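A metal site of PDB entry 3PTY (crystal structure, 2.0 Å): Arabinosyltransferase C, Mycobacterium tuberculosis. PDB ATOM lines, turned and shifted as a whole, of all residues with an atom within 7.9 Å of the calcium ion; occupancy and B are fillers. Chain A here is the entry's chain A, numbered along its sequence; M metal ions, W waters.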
ATOM      1  N   SER A 135     -17.043 -31.682  27.840  1.00  0.00           N
ATOM      2  CA  SER A 135     -18.499 -31.813  27.827  1.00  0.00           C
ATOM      3  C   SER A 135     -19.042 -32.375  26.518  1.00  0.00           C
ATOM      4  O   SER A 135     -20.251 -32.368  26.299  1.00  0.00           O
ATOM      5  CB  SER A 135     -19.160 -30.467  28.100  1.00  0.00           C
ATOM      6  OG  SER A 135     -18.871 -29.551  27.061  1.00  0.00           O
ATOM      7  N   TRP A 136     -18.161 -32.862  25.633  1.00  0.00           N
ATOM      8  CA  TRP A 136     -18.649 -33.465  24.401  1.00  0.00           C
ATOM      9  C   TRP A 136     -19.260 -34.834  24.682  1.00  0.00           C
ATOM     10  O   TRP A 136     -18.798 -35.560  25.563  1.00  0.00           O
ATOM     11  CB  TRP A 136     -17.543 -33.616  23.359  1.00  0.00           C
ATOM     12  CG  TRP A 136     -18.027 -34.337  22.130  1.00  0.00           C
ATOM     13  CD1 TRP A 136     -18.610 -33.785  21.023  1.00  0.00           C
ATOM     14  CD2 TRP A 136     -17.991 -35.757  21.887  1.00  0.00           C
ATOM     15  NE1 TRP A 136     -18.922 -34.766  20.110  1.00  0.00           N
ATOM     16  CE2 TRP A 136     -18.556 -35.979  20.617  1.00  0.00           C
ATOM     17  CE3 TRP A 136     -17.525 -36.843  22.621  1.00  0.00           C
ATOM     18  CZ2 TRP A 136     -18.673 -37.257  20.070  1.00  0.00           C
ATOM     19  CZ3 TRP A 136     -17.642 -38.121  22.074  1.00  0.00           C
ATOM     20  CH2 TRP A 136     -18.210 -38.316  20.811  1.00  0.00           C
ATOM     21  N   ARG A 137     -20.294 -35.176  23.922  1.00  0.00           N
ATOM     22  CA  ARG A 137     -20.835 -36.528  23.932  1.00  0.00           C
ATOM     23  C   ARG A 137     -21.614 -36.802  22.660  1.00  0.00           C
ATOM     24  O   ARG A 137     -22.101 -35.878  22.003  1.00  0.00           O
ATOM     25  CB  ARG A 137     -21.715 -36.759  25.164  1.00  0.00           C
ATOM     26  CG  ARG A 137     -22.991 -35.917  25.188  1.00  0.00           C
ATOM     27  CD  ARG A 137     -23.698 -36.069  26.526  1.00  0.00           C
ATOM     28  NE  ARG A 137     -22.753 -35.907  27.633  1.00  0.00           N
ATOM     29  CZ  ARG A 137     -22.923 -36.423  28.848  1.00  0.00           C
ATOM     30  NH1 ARG A 137     -24.000 -37.143  29.117  1.00  0.00           N
ATOM     31  NH2 ARG A 137     -22.008 -36.222  29.781  1.00  0.00           N
ATOM     32  N   GLN A 141     -27.815 -34.725  23.956  1.00  0.00           N
ATOM     33  CA  GLN A 141     -27.045 -33.628  24.514  1.00  0.00           C
ATOM     34  C   GLN A 141     -27.658 -33.150  25.826  1.00  0.00           C
ATOM     35  O   GLN A 141     -28.874 -33.040  25.931  1.00  0.00           O
ATOM     36  CB  GLN A 141     -26.962 -32.487  23.516  1.00  0.00           C
ATOM     37  CG  GLN A 141     -26.354 -32.894  22.180  1.00  0.00           C
ATOM     38  CD  GLN A 141     -24.941 -33.400  22.336  1.00  0.00           C
ATOM     39  OE1 GLN A 141     -24.048 -32.672  22.787  1.00  0.00           O
ATOM     40  NE2 GLN A 141     -24.708 -34.659  21.968  1.00  0.00           N
ATOM     41  N   VAL A 142     -26.818 -32.864  26.817  1.00  0.00           N
ATOM     42  CA  VAL A 142     -27.299 -32.407  28.113  1.00  0.00           C
ATOM     43  C   VAL A 142     -26.530 -31.155  28.574  1.00  0.00           C
ATOM     44  O   VAL A 142     -25.428 -30.900  28.091  1.00  0.00           O
ATOM     45  CB  VAL A 142     -27.151 -33.497  29.184  1.00  0.00           C
ATOM     46  CG1 VAL A 142     -27.909 -34.762  28.750  1.00  0.00           C
ATOM     47  CG2 VAL A 142     -25.684 -33.817  29.420  1.00  0.00           C
ATOM     48  N   PRO A 143     -27.118 -30.377  29.490  1.00  0.00           N
ATOM     49  CA  PRO A 143     -26.416 -29.214  30.040  1.00  0.00           C
ATOM     50  C   PRO A 143     -25.173 -29.667  30.801  1.00  0.00           C
ATOM     51  O   PRO A 143     -25.182 -30.735  31.396  1.00  0.00           O
ATOM     52  CB  PRO A 143     -27.432 -28.614  31.014  1.00  0.00           C
ATOM     53  CG  PRO A 143     -28.755 -29.146  30.587  1.00  0.00           C
ATOM     54  CD  PRO A 143     -28.495 -30.507  30.028  1.00  0.00           C
ATOM     55  N   ALA A 144     -24.117 -28.857  30.781  1.00  0.00           N
ATOM     56  CA  ALA A 144     -22.874 -29.253  31.432  1.00  0.00           C
ATOM     57  C   ALA A 144     -22.221 -28.060  32.096  1.00  0.00           C
ATOM     58  O   ALA A 144     -22.323 -26.927  31.618  1.00  0.00           O
ATOM     59  CB  ALA A 144     -21.925 -29.898  30.422  1.00  0.00           C
ATOM     60  N   ARG A 172     -15.904 -25.696  20.912  1.00  0.00           N
ATOM     61  CA  ARG A 172     -16.442 -24.442  20.409  1.00  0.00           C
ATOM     62  C   ARG A 172     -17.257 -23.799  21.500  1.00  0.00           C
ATOM     63  O   ARG A 172     -18.223 -24.376  21.999  1.00  0.00           O
ATOM     64  CB  ARG A 172     -17.339 -24.673  19.189  1.00  0.00           C
ATOM     65  CG  ARG A 172     -16.651 -25.358  18.017  1.00  0.00           C
ATOM     66  CD  ARG A 172     -17.625 -25.448  16.837  1.00  0.00           C
ATOM     67  NE  ARG A 172     -17.110 -26.312  15.783  1.00  0.00           N
ATOM     68  CZ  ARG A 172     -17.078 -27.643  15.860  1.00  0.00           C
ATOM     69  NH1 ARG A 172     -17.512 -28.254  16.952  1.00  0.00           N
ATOM     70  NH2 ARG A 172     -16.606 -28.355  14.846  1.00  0.00           N
ATOM     71  N   GLU A 177     -18.185 -18.275  28.334  1.00  0.00           N
ATOM     72  CA  GLU A 177     -18.486 -19.615  28.851  1.00  0.00           C
ATOM     73  C   GLU A 177     -17.349 -20.236  29.665  1.00  0.00           C
ATOM     74  O   GLU A 177     -17.550 -21.246  30.333  1.00  0.00           O
ATOM     75  CB  GLU A 177     -18.872 -20.566  27.715  1.00  0.00           C
ATOM     76  CG  GLU A 177     -20.226 -20.280  27.089  1.00  0.00           C
ATOM     77  CD  GLU A 177     -20.501 -21.180  25.903  1.00  0.00           C
ATOM     78  OE1 GLU A 177     -20.973 -22.314  26.113  1.00  0.00           O
ATOM     79  OE2 GLU A 177     -20.250 -20.750  24.754  1.00  0.00           O
ATOM     80  N   ASP A 230     -19.302 -23.187  31.583  1.00  0.00           N
ATOM     81  CA  ASP A 230     -20.738 -23.383  31.491  1.00  0.00           C
ATOM     82  C   ASP A 230     -21.083 -23.693  30.048  1.00  0.00           C
ATOM     83  O   ASP A 230     -20.889 -22.856  29.154  1.00  0.00           O
ATOM     84  CB  ASP A 230     -21.468 -22.121  31.977  1.00  0.00           C
ATOM     85  CG  ASP A 230     -22.957 -22.345  32.142  1.00  0.00           C
ATOM     86  OD1 ASP A 230     -23.385 -23.520  32.245  1.00  0.00           O
ATOM     87  OD2 ASP A 230     -23.706 -21.347  32.165  1.00  0.00           O
ATOM     88  N   ASP A 231     -21.574 -24.904  29.818  1.00  0.00           N
ATOM     89  CA  ASP A 231     -21.952 -25.334  28.484  1.00  0.00           C
ATOM     90  C   ASP A 231     -23.416 -25.746  28.447  1.00  0.00           C
ATOM     91  O   ASP A 231     -23.755 -26.931  28.581  1.00  0.00           O
ATOM     92  CB  ASP A 231     -21.057 -26.489  28.049  1.00  0.00           C
ATOM     93  CG  ASP A 231     -21.481 -27.077  26.733  1.00  0.00           C
ATOM     94  OD1 ASP A 231     -22.293 -26.430  26.030  1.00  0.00           O
ATOM     95  OD2 ASP A 231     -20.999 -28.173  26.391  1.00  0.00           O
ATOM     96  N   GLN A 232     -24.278 -24.741  28.256  1.00  0.00           N
ATOM     97  CA  GLN A 232     -25.726 -24.928  28.240  1.00  0.00           C
ATOM     98  C   GLN A 232     -26.256 -25.099  26.814  1.00  0.00           C
ATOM     99  O   GLN A 232     -27.448 -25.338  26.618  1.00  0.00           O
ATOM    100  CB  GLN A 232     -26.409 -23.726  28.872  1.00  0.00           C
ATOM    101  CG  GLN A 232     -26.044 -23.496  30.326  1.00  0.00           C
ATOM    102  CD  GLN A 232     -26.570 -24.589  31.231  1.00  0.00           C
ATOM    103  OE1 GLN A 232     -27.715 -25.014  31.101  1.00  0.00           O
ATOM    104  NE2 GLN A 232     -25.739 -25.047  32.162  1.00  0.00           N
ATOM    105  N   ASP A 233     -25.380 -24.945  25.833  1.00  0.00           N
ATOM    106  CA  ASP A 233     -25.781 -25.018  24.439  1.00  0.00           C
ATOM    107  C   ASP A 233     -25.823 -26.471  23.989  1.00  0.00           C
ATOM    108  O   ASP A 233     -24.798 -27.131  23.948  1.00  0.00           O
ATOM    109  CB  ASP A 233     -24.804 -24.224  23.578  1.00  0.00           C
ATOM    110  CG  ASP A 233     -25.189 -24.194  22.104  1.00  0.00           C
ATOM    111  OD1 ASP A 233     -25.983 -25.051  21.666  1.00  0.00           O
ATOM    112  OD2 ASP A 233     -24.670 -23.315  21.377  1.00  0.00           O
ATOM    113  N   LEU A 234     -27.010 -26.968  23.650  1.00  0.00           N
ATOM    114  CA  LEU A 234     -27.190 -28.387  23.395  1.00  0.00           C
ATOM    115  C   LEU A 234     -26.909 -28.806  21.952  1.00  0.00           C
ATOM    116  O   LEU A 234     -27.046 -29.978  21.617  1.00  0.00           O
ATOM    117  CB  LEU A 234     -28.588 -28.837  23.818  1.00  0.00           C
ATOM    118  CG  LEU A 234     -28.939 -28.519  25.275  1.00  0.00           C
ATOM    119  CD1 LEU A 234     -30.350 -28.966  25.587  1.00  0.00           C
ATOM    120  CD2 LEU A 234     -27.935 -29.162  26.219  1.00  0.00           C
ATOM    121  N   ALA A 235     -26.529 -27.864  21.097  1.00  0.00           N
ATOM    122  CA  ALA A 235     -26.035 -28.225  19.782  1.00  0.00           C
ATOM    123  C   ALA A 235     -24.798 -29.110  19.967  1.00  0.00           C
ATOM    124  O   ALA A 235     -23.913 -28.771  20.740  1.00  0.00           O
ATOM    125  CB  ALA A 235     -25.689 -26.997  18.966  1.00  0.00           C
ATOM    126  N   PRO A 236     -24.753 -30.244  19.254  1.00  0.00           N
ATOM    127  CA  PRO A 236     -23.697 -31.256  19.437  1.00  0.00           C
ATOM    128  C   PRO A 236     -22.307 -30.681  19.219  1.00  0.00           C
ATOM    129  O   PRO A 236     -21.351 -31.124  19.864  1.00  0.00           O
ATOM    130  CB  PRO A 236     -24.018 -32.290  18.347  1.00  0.00           C
ATOM    131  CG  PRO A 236     -25.481 -32.136  18.103  1.00  0.00           C
ATOM    132  CD  PRO A 236     -25.745 -30.665  18.245  1.00  0.00           C
ATOM    133  N   GLN A 237     -22.192 -29.708  18.323  1.00  0.00           N
ATOM    134  CA  GLN A 237     -20.904 -29.133  17.960  1.00  0.00           C
ATOM    135  C   GLN A 237     -20.404 -28.155  19.021  1.00  0.00           C
ATOM    136  O   GLN A 237     -19.245 -27.738  18.983  1.00  0.00           O
ATOM    137  CB  GLN A 237     -21.001 -28.428  16.598  1.00  0.00           C
ATOM    138  N   HIS A 238     -21.270 -27.790  19.958  1.00  0.00           N
ATOM    139  CA  HIS A 238     -20.914 -26.822  20.978  1.00  0.00           C
ATOM    140  C   HIS A 238     -20.531 -27.552  22.246  1.00  0.00           C
ATOM    141  O   HIS A 238     -21.393 -28.029  22.965  1.00  0.00           O
ATOM    142  CB  HIS A 238     -22.074 -25.867  21.234  1.00  0.00           C
ATOM    143  CG  HIS A 238     -21.690 -24.654  22.020  1.00  0.00           C
ATOM    144  ND1 HIS A 238     -21.475 -23.426  21.433  1.00  0.00           N
ATOM    145  CD2 HIS A 238     -21.482 -24.473  23.343  1.00  0.00           C
ATOM    146  CE1 HIS A 238     -21.163 -22.536  22.356  1.00  0.00           C
ATOM    147  NE2 HIS A 238     -21.155 -23.143  23.533  1.00  0.00           N
ATOM    148  N   TRP A 239     -19.226 -27.652  22.507  1.00  0.00           N
ATOM    149  CA  TRP A 239     -18.751 -28.362  23.689  1.00  0.00           C
ATOM    150  C   TRP A 239     -17.423 -27.761  24.133  1.00  0.00           C
ATOM    151  O   TRP A 239     -16.802 -26.984  23.403  1.00  0.00           O
ATOM    152  CB  TRP A 239     -18.585 -29.859  23.385  1.00  0.00           C
ATOM    153  CG  TRP A 239     -17.748 -30.131  22.173  1.00  0.00           C
ATOM    154  CD1 TRP A 239     -18.179 -30.249  20.885  1.00  0.00           C
ATOM    155  CD2 TRP A 239     -16.326 -30.296  22.140  1.00  0.00           C
ATOM    156  NE1 TRP A 239     -17.119 -30.488  20.053  1.00  0.00           N
ATOM    157  CE2 TRP A 239     -15.964 -30.513  20.788  1.00  0.00           C
ATOM    158  CE3 TRP A 239     -15.317 -30.273  23.106  1.00  0.00           C
ATOM    159  CZ2 TRP A 239     -14.642 -30.719  20.393  1.00  0.00           C
ATOM    160  CZ3 TRP A 239     -14.009 -30.482  22.712  1.00  0.00           C
ATOM    161  CH2 TRP A 239     -13.683 -30.698  21.363  1.00  0.00           C
ATOM    162  N   ILE A 240     -16.987 -28.115  25.341  1.00  0.00           N
ATOM    163  CA  ILE A 240     -15.791 -27.540  25.934  1.00  0.00           C
ATOM    164  C   ILE A 240     -14.927 -28.633  26.569  1.00  0.00           C
ATOM    165  O   ILE A 240     -15.451 -29.501  27.248  1.00  0.00           O
ATOM    166  CB  ILE A 240     -16.152 -26.536  27.048  1.00  0.00           C
ATOM    167  CG1 ILE A 240     -17.114 -25.462  26.521  1.00  0.00           C
ATOM    168  CG2 ILE A 240     -14.890 -25.881  27.624  1.00  0.00           C
ATOM    169  CD1 ILE A 240     -17.671 -24.546  27.611  1.00  0.00           C
HETATM  170 CA    CA M   1     -22.938 -28.598  24.704  1.00  0.00          CA
HETATM  171  O   HOH W   1     -24.212 -30.064  23.031  1.00  0.00           O
HETATM  172  O   HOH W   2     -24.219 -28.974  26.824  1.00  0.00           O
HETATM  173  O   HOH W   3     -21.812 -30.981  24.878  1.00  0.00           O
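Three residues have an atom within 4 Å of the calcium ion: Asp 231, Asp 233 and His 238.
The nearest printed residue that does not touch the calcium ion is Ala 235 (4.1 Å).
The calcium ion is bound by O of His 238 (2.4 Å), O of Asp 233 (2.5 Å), water W2 (2.5 Å), water W1 (2.6 Å), OD2 of Asp 231 (2.6 Å), OD1 of Asp 231 (2.6 Å) and water W3 (2.6 Å).
The calcium ion has seven donor atoms within binding distance.
A ring nitrogen (NE2) of His 238 sits at hydrogen-bond distance from the side-chain carboxylate of Glu 177, at 2.7 Å.
ND1 of His 238 sits at hydrogen-bond distance from O of Arg 172.
The side-chain carboxylate (OD1) of Asp 233 lies within hydrogen-bond range of the backbone NH (N) of Ala 235, 2.9 Å away.
The side-chain carboxylate of Asp 231 lies close to the side-chain hydroxyl of Ser 135 (2.6 Å).
The backbone carbonyl oxygen (O) of Ala 144 lies within hydrogen-bond range of the backbone NH (N) of Asp 231, 2.8 Å away.
Water W3 lies within hydrogen-bond range of O of Ser 135 and OE1 of Gln 141.
Water W2 lies within hydrogen-bond range of the backbone carbonyl oxygen (O) of Val 142 (2.6 Å) and the backbone carbonyl oxygen (O) of Asp 231 (2.7 Å).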
